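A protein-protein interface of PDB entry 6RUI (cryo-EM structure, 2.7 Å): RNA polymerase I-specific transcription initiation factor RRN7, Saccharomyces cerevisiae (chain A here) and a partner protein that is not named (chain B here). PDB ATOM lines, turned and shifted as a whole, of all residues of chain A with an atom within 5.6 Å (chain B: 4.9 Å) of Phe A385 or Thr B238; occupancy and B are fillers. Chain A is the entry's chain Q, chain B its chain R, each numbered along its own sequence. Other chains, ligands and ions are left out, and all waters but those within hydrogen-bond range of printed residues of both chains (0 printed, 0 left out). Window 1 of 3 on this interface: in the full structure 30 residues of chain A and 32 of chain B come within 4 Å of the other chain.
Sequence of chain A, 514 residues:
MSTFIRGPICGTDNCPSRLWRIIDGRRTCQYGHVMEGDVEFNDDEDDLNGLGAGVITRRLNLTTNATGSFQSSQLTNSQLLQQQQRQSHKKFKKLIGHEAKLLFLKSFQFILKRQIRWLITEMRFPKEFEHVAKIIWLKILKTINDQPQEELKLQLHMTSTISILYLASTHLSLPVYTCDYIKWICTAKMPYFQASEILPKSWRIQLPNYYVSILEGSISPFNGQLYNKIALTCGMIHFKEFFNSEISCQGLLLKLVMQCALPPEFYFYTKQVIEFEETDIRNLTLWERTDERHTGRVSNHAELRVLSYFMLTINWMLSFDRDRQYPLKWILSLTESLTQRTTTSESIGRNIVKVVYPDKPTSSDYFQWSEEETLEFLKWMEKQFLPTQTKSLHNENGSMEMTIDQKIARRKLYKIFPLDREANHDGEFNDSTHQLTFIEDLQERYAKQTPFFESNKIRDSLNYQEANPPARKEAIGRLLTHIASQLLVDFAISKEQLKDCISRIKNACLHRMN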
ATOM      1  N   LEU A 378      25.513 -14.956   1.250  1.00  0.00           N
ATOM      2  CA  LEU A 378      25.723 -13.663   0.620  1.00  0.00           C
ATOM      3  C   LEU A 378      27.195 -13.379   0.387  1.00  0.00           C
ATOM      4  O   LEU A 378      27.534 -12.661  -0.557  1.00  0.00           O
ATOM      5  CB  LEU A 378      25.091 -12.558   1.455  1.00  0.00           C
ATOM      6  CG  LEU A 378      23.565 -12.586   1.462  1.00  0.00           C
ATOM      7  CD1 LEU A 378      23.035 -11.554   2.409  1.00  0.00           C
ATOM      8  CD2 LEU A 378      23.016 -12.362   0.072  1.00  0.00           C
ATOM      9  N   MET A 381      27.738 -14.921  -2.685  1.00  0.00           N
ATOM     10  CA  MET A 381      27.209 -14.123  -3.790  1.00  0.00           C
ATOM     11  C   MET A 381      28.231 -13.131  -4.320  1.00  0.00           C
ATOM     12  O   MET A 381      28.196 -12.786  -5.503  1.00  0.00           O
ATOM     13  CB  MET A 381      25.954 -13.374  -3.361  1.00  0.00           C
ATOM     14  CG  MET A 381      24.765 -14.251  -3.126  1.00  0.00           C
ATOM     15  SD  MET A 381      24.335 -15.139  -4.614  1.00  0.00           S
ATOM     16  CE  MET A 381      23.800 -13.778  -5.620  1.00  0.00           C
ATOM     17  N   GLU A 382      29.169 -12.698  -3.480  1.00  0.00           N
ATOM     18  CA  GLU A 382      30.270 -11.884  -3.974  1.00  0.00           C
ATOM     19  C   GLU A 382      31.244 -12.697  -4.819  1.00  0.00           C
ATOM     20  O   GLU A 382      32.073 -12.118  -5.529  1.00  0.00           O
ATOM     21  CB  GLU A 382      30.994 -11.232  -2.808  1.00  0.00           C
ATOM     22  CG  GLU A 382      30.139 -10.266  -2.043  1.00  0.00           C
ATOM     23  CD  GLU A 382      30.905  -9.603  -0.932  1.00  0.00           C
ATOM     24  OE1 GLU A 382      32.069  -9.993  -0.713  1.00  0.00           O
ATOM     25  OE2 GLU A 382      30.355  -8.694  -0.275  1.00  0.00           O
ATOM     26  N   LYS A 383      31.190 -14.026  -4.733  1.00  0.00           N
ATOM     27  CA  LYS A 383      31.861 -14.890  -5.692  1.00  0.00           C
ATOM     28  C   LYS A 383      30.909 -15.336  -6.818  1.00  0.00           C
ATOM     29  O   LYS A 383      31.241 -16.223  -7.609  1.00  0.00           O
ATOM     30  CB  LYS A 383      32.474 -16.082  -4.946  1.00  0.00           C
ATOM     31  CG  LYS A 383      33.622 -16.811  -5.646  1.00  0.00           C
ATOM     32  CD  LYS A 383      34.158 -17.939  -4.798  1.00  0.00           C
ATOM     33  CE  LYS A 383      35.401 -17.504  -4.048  1.00  0.00           C
ATOM     34  NZ  LYS A 383      35.092 -16.633  -2.886  1.00  0.00           N
ATOM     35  N   GLN A 384      29.722 -14.741  -6.916  1.00  0.00           N
ATOM     36  CA  GLN A 384      28.935 -14.846  -8.138  1.00  0.00           C
ATOM     37  C   GLN A 384      29.089 -13.632  -9.043  1.00  0.00           C
ATOM     38  O   GLN A 384      29.076 -13.792 -10.268  1.00  0.00           O
ATOM     39  CB  GLN A 384      27.449 -15.077  -7.815  1.00  0.00           C
ATOM     40  CG  GLN A 384      26.521 -15.154  -9.039  1.00  0.00           C
ATOM     41  CD  GLN A 384      25.153 -15.705  -8.744  1.00  0.00           C
ATOM     42  OE1 GLN A 384      24.876 -16.130  -7.637  1.00  0.00           O
ATOM     43  NE2 GLN A 384      24.283 -15.698  -9.744  1.00  0.00           N
ATOM     44  N   PHE A 385      29.309 -12.436  -8.478  1.00  0.00           N
ATOM     45  CA  PHE A 385      29.300 -11.222  -9.292  1.00  0.00           C
ATOM     46  C   PHE A 385      30.473 -11.168 -10.250  1.00  0.00           C
ATOM     47  O   PHE A 385      30.328 -10.704 -11.386  1.00  0.00           O
ATOM     48  CB  PHE A 385      29.329  -9.972  -8.429  1.00  0.00           C
ATOM     49  CG  PHE A 385      28.130  -9.802  -7.590  1.00  0.00           C
ATOM     50  CD1 PHE A 385      26.894  -9.639  -8.176  1.00  0.00           C
ATOM     51  CD2 PHE A 385      28.245  -9.704  -6.221  1.00  0.00           C
ATOM     52  CE1 PHE A 385      25.785  -9.465  -7.407  1.00  0.00           C
ATOM     53  CE2 PHE A 385      27.138  -9.522  -5.447  1.00  0.00           C
ATOM     54  CZ  PHE A 385      25.909  -9.401  -6.044  1.00  0.00           C
ATOM     55  N   LEU A 386      31.631 -11.616  -9.813  1.00  0.00           N
ATOM     56  CA  LEU A 386      32.782 -11.591 -10.697  1.00  0.00           C
ATOM     57  C   LEU A 386      32.648 -12.630 -11.813  1.00  0.00           C
ATOM     58  O   LEU A 386      33.047 -12.328 -12.943  1.00  0.00           O
ATOM     59  CB  LEU A 386      34.091 -11.767  -9.914  1.00  0.00           C
ATOM     60  CG  LEU A 386      34.611 -10.572  -9.099  1.00  0.00           C
ATOM     61  CD1 LEU A 386      33.923 -10.447  -7.730  1.00  0.00           C
ATOM     62  CD2 LEU A 386      36.135 -10.590  -8.957  1.00  0.00           C
ATOM     63  N   PRO A 387      32.089 -13.861 -11.587  1.00  0.00           N
ATOM     64  CA  PRO A 387      31.722 -14.671 -12.753  1.00  0.00           C
ATOM     65  C   PRO A 387      30.491 -14.174 -13.491  1.00  0.00           C
ATOM     66  O   PRO A 387      30.442 -14.247 -14.721  1.00  0.00           O
ATOM     67  CB  PRO A 387      31.479 -16.059 -12.156  1.00  0.00           C
ATOM     68  CG  PRO A 387      32.282 -16.091 -10.963  1.00  0.00           C
ATOM     69  CD  PRO A 387      32.190 -14.730 -10.396  1.00  0.00           C
ATOM     70  N   THR A 388      29.492 -13.679 -12.770  1.00  0.00           N
ATOM     71  CA  THR A 388      28.257 -13.251 -13.420  1.00  0.00           C
ATOM     72  C   THR A 388      28.019 -11.752 -13.238  1.00  0.00           C
ATOM     73  O   THR A 388      28.439 -10.935 -14.060  1.00  0.00           O
ATOM     74  CB  THR A 388      27.043 -14.025 -12.875  1.00  0.00           C
ATOM     75  OG1 THR A 388      27.276 -15.432 -13.006  1.00  0.00           O
ATOM     76  CG2 THR A 388      25.795 -13.657 -13.651  1.00  0.00           C
ATOM     77  N   LEU A 419      28.216  -2.217  -2.076  1.00  0.00           N
ATOM     78  CA  LEU A 419      28.007  -3.662  -2.075  1.00  0.00           C
ATOM     79  C   LEU A 419      28.396  -4.285  -0.748  1.00  0.00           C
ATOM     80  O   LEU A 419      27.756  -5.243  -0.304  1.00  0.00           O
ATOM     81  CB  LEU A 419      28.788  -4.296  -3.228  1.00  0.00           C
ATOM     82  CG  LEU A 419      28.695  -5.783  -3.603  1.00  0.00           C
ATOM     83  CD1 LEU A 419      29.722  -6.645  -2.880  1.00  0.00           C
ATOM     84  CD2 LEU A 419      27.290  -6.316  -3.342  1.00  0.00           C
ATOM     85  N   LEU B 216      16.712 -14.900  -4.170  1.00  0.00           N
ATOM     86  CA  LEU B 216      17.004 -13.678  -3.438  1.00  0.00           C
ATOM     87  C   LEU B 216      15.741 -12.903  -3.096  1.00  0.00           C
ATOM     88  O   LEU B 216      15.643 -12.336  -2.005  1.00  0.00           O
ATOM     89  CB  LEU B 216      17.979 -12.820  -4.224  1.00  0.00           C
ATOM     90  CG  LEU B 216      19.372 -13.414  -4.154  1.00  0.00           C
ATOM     91  CD1 LEU B 216      20.293 -12.610  -4.998  1.00  0.00           C
ATOM     92  CD2 LEU B 216      19.846 -13.440  -2.721  1.00  0.00           C
ATOM     93  N   LYS B 234      21.483  -6.285   2.635  1.00  0.00           N
ATOM     94  CA  LYS B 234      22.544  -6.997   1.943  1.00  0.00           C
ATOM     95  C   LYS B 234      21.998  -7.794   0.776  1.00  0.00           C
ATOM     96  O   LYS B 234      22.659  -7.911  -0.257  1.00  0.00           O
ATOM     97  CB  LYS B 234      23.280  -7.914   2.909  1.00  0.00           C
ATOM     98  CG  LYS B 234      24.060  -7.201   3.969  1.00  0.00           C
ATOM     99  CD  LYS B 234      24.779  -8.190   4.855  1.00  0.00           C
ATOM    100  CE  LYS B 234      25.414  -7.497   6.036  1.00  0.00           C
ATOM    101  NZ  LYS B 234      26.498  -6.585   5.602  1.00  0.00           N
ATOM    102  N   ILE B 235      20.791  -8.334   0.914  1.00  0.00           N
ATOM    103  CA  ILE B 235      20.168  -9.037  -0.198  1.00  0.00           C
ATOM    104  C   ILE B 235      19.776  -8.054  -1.288  1.00  0.00           C
ATOM    105  O   ILE B 235      19.928  -8.335  -2.483  1.00  0.00           O
ATOM    106  CB  ILE B 235      18.966  -9.842   0.314  1.00  0.00           C
ATOM    107  CG1 ILE B 235      19.453 -10.908   1.277  1.00  0.00           C
ATOM    108  CG2 ILE B 235      18.207 -10.488  -0.807  1.00  0.00           C
ATOM    109  CD1 ILE B 235      18.358 -11.551   2.030  1.00  0.00           C
ATOM    110  N   PHE B 236      19.327  -6.864  -0.896  1.00  0.00           N
ATOM    111  CA  PHE B 236      18.864  -5.897  -1.882  1.00  0.00           C
ATOM    112  C   PHE B 236      20.022  -5.261  -2.632  1.00  0.00           C
ATOM    113  O   PHE B 236      19.877  -4.916  -3.806  1.00  0.00           O
ATOM    114  CB  PHE B 236      18.015  -4.831  -1.202  1.00  0.00           C
ATOM    115  CG  PHE B 236      17.350  -3.903  -2.154  1.00  0.00           C
ATOM    116  CD1 PHE B 236      16.285  -4.331  -2.902  1.00  0.00           C
ATOM    117  CD2 PHE B 236      17.791  -2.611  -2.313  1.00  0.00           C
ATOM    118  CE1 PHE B 236      15.667  -3.484  -3.778  1.00  0.00           C
ATOM    119  CE2 PHE B 236      17.173  -1.768  -3.198  1.00  0.00           C
ATOM    120  CZ  PHE B 236      16.107  -2.204  -3.923  1.00  0.00           C
ATOM    121  N   ALA B 237      21.173  -5.103  -1.981  1.00  0.00           N
ATOM    122  CA  ALA B 237      22.352  -4.608  -2.678  1.00  0.00           C
ATOM    123  C   ALA B 237      22.901  -5.642  -3.642  1.00  0.00           C
ATOM    124  O   ALA B 237      23.488  -5.283  -4.667  1.00  0.00           O
ATOM    125  CB  ALA B 237      23.426  -4.206  -1.674  1.00  0.00           C
ATOM    126  N   THR B 238      22.722  -6.922  -3.336  1.00  0.00           N
ATOM    127  CA  THR B 238      23.189  -7.966  -4.235  1.00  0.00           C
ATOM    128  C   THR B 238      22.218  -8.237  -5.371  1.00  0.00           C
ATOM    129  O   THR B 238      22.635  -8.693  -6.437  1.00  0.00           O
ATOM    130  CB  THR B 238      23.431  -9.258  -3.468  1.00  0.00           C
ATOM    131  OG1 THR B 238      22.255  -9.594  -2.735  1.00  0.00           O
ATOM    132  CG2 THR B 238      24.605  -9.109  -2.540  1.00  0.00           C
ATOM    133  N   LEU B 239      20.931  -7.984  -5.160  1.00  0.00           N
ATOM    134  CA  LEU B 239      19.944  -8.282  -6.186  1.00  0.00           C
ATOM    135  C   LEU B 239      19.979  -7.267  -7.316  1.00  0.00           C
ATOM    136  O   LEU B 239      19.740  -7.624  -8.471  1.00  0.00           O
ATOM    137  CB  LEU B 239      18.560  -8.326  -5.550  1.00  0.00           C
ATOM    138  CG  LEU B 239      17.332  -8.610  -6.396  1.00  0.00           C
ATOM    139  CD1 LEU B 239      17.385  -9.996  -6.993  1.00  0.00           C
ATOM    140  CD2 LEU B 239      16.124  -8.443  -5.521  1.00  0.00           C
ATOM    141  N   ILE B 240      20.279  -6.003  -7.013  1.00  0.00           N
ATOM    142  CA  ILE B 240      20.284  -4.969  -8.038  1.00  0.00           C
ATOM    143  C   ILE B 240      21.505  -5.060  -8.931  1.00  0.00           C
ATOM    144  O   ILE B 240      21.525  -4.459 -10.008  1.00  0.00           O
ATOM    145  CB  ILE B 240      20.192  -3.583  -7.384  1.00  0.00           C
ATOM    146  CG1 ILE B 240      21.355  -3.384  -6.421  1.00  0.00           C
ATOM    147  CG2 ILE B 240      18.896  -3.440  -6.659  1.00  0.00           C
ATOM    148  CD1 ILE B 240      21.414  -2.027  -5.803  1.00  0.00           C
ATOM    149  N   ARG B 241      22.525  -5.798  -8.514  1.00  0.00           N
ATOM    150  CA  ARG B 241      23.739  -5.964  -9.289  1.00  0.00           C
ATOM    151  C   ARG B 241      23.686  -7.153 -10.224  1.00  0.00           C
ATOM    152  O   ARG B 241      24.508  -7.238 -11.138  1.00  0.00           O
ATOM    153  CB  ARG B 241      24.927  -6.107  -8.349  1.00  0.00           C
ATOM    154  CG  ARG B 241      25.300  -4.806  -7.716  1.00  0.00           C
ATOM    155  CD  ARG B 241      26.398  -4.938  -6.709  1.00  0.00           C
ATOM    156  NE  ARG B 241      26.903  -3.637  -6.298  1.00  0.00           N
ATOM    157  CZ  ARG B 241      26.365  -2.892  -5.345  1.00  0.00           C
ATOM    158  NH1 ARG B 241      26.910  -1.729  -5.039  1.00  0.00           N
ATOM    159  NH2 ARG B 241      25.285  -3.299  -4.707  1.00  0.00           N
ATOM    160  N   ILE B 242      22.754  -8.063 -10.016  1.00  0.00           N
ATOM    161  CA  ILE B 242      22.588  -9.196 -10.922  1.00  0.00           C
ATOM    162  C   ILE B 242      21.810  -8.724 -12.144  1.00  0.00           C
ATOM    163  O   ILE B 242      20.740  -8.120 -11.979  1.00  0.00           O
ATOM    164  CB  ILE B 242      21.867 -10.326 -10.218  1.00  0.00           C
ATOM    165  CG1 ILE B 242      22.704 -10.822  -9.059  1.00  0.00           C
ATOM    166  CG2 ILE B 242      21.599 -11.464 -11.158  1.00  0.00           C
ATOM    167  CD1 ILE B 242      21.972 -11.755  -8.189  1.00  0.00           C
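The backbone NH of Leu A419 lies close to the guanidinium group of Arg B241 (3.3 Å).
CD1 of Leu A378 touches CB of Lys B234, 3.7 Å away.
Leu A378 touches Ile B235 (CD1 to CG1, 3.8 Å).
CE of Met A381 touches CD1 of Leu B216, at 3.7 Å.
Ile B242 touches Met A381 (CD1 to CE, 3.7 Å).
Phe A385 touches Thr B238 (CZ to O, 3.4 Å).
CE1 of Phe A385 touches CB of Arg B241, at 3.6 Å.
Phe A385 touches Ile B242 (CE1 to CG1, 3.8 Å).
Leu A419 touches Thr B238.
Of the 10 printed residues of chain B, 6 touch a printed residue of chain A.
Hydrophobic or aromatic side chains of chain B within 4 Å of the printed part of chain A: Leu B216, Ile B235 and Ile B242.
Phe A385 touches just these residues of chain B: Thr B238 (3.4 Å), Arg B241 (3.6 Å) and Ile B242 (3.8 Å).
Printed residues of chain A within 4 Å of Thr B238: Phe A385 and Leu A419.
Of the printed residues of chain A, Ile B242 touches Met A381 and Phe A385.
Of the printed residues of chain A, Leu B216 touches Met A381.
Of the printed residues of chain A, Lys B234 touches Leu A378.
Of the printed residues of chain B, Leu A378 touches Lys B234 (3.7 Å) and Ile B235 (3.8 Å).
The nearest printed residue of chain A that does not touch Thr B238 is Leu A378 (4.01 Å).
The nearest printed residue of chain A that does not touch Ile B235 is Phe A385 (7.0 Å).
The side-chain sulfur (SD) of Met A381 lies close to the side-chain amide oxygen (OE1) of Gln A384 (3.2 Å).
The backbone carbonyl oxygen of Lys B234 lies within hydrogen-bond range of the side-chain hydroxyl of Thr B238, at 3.0 Å.
The backbone carbonyl oxygen (O) of Ile B235 sits at hydrogen-bond distance from the side-chain hydroxyl (OG1) of Thr B238, at 2.7 Å.
O of Ala B237 is in hydrogen-bond range of NH2 of Arg B241 (2.7 Å).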
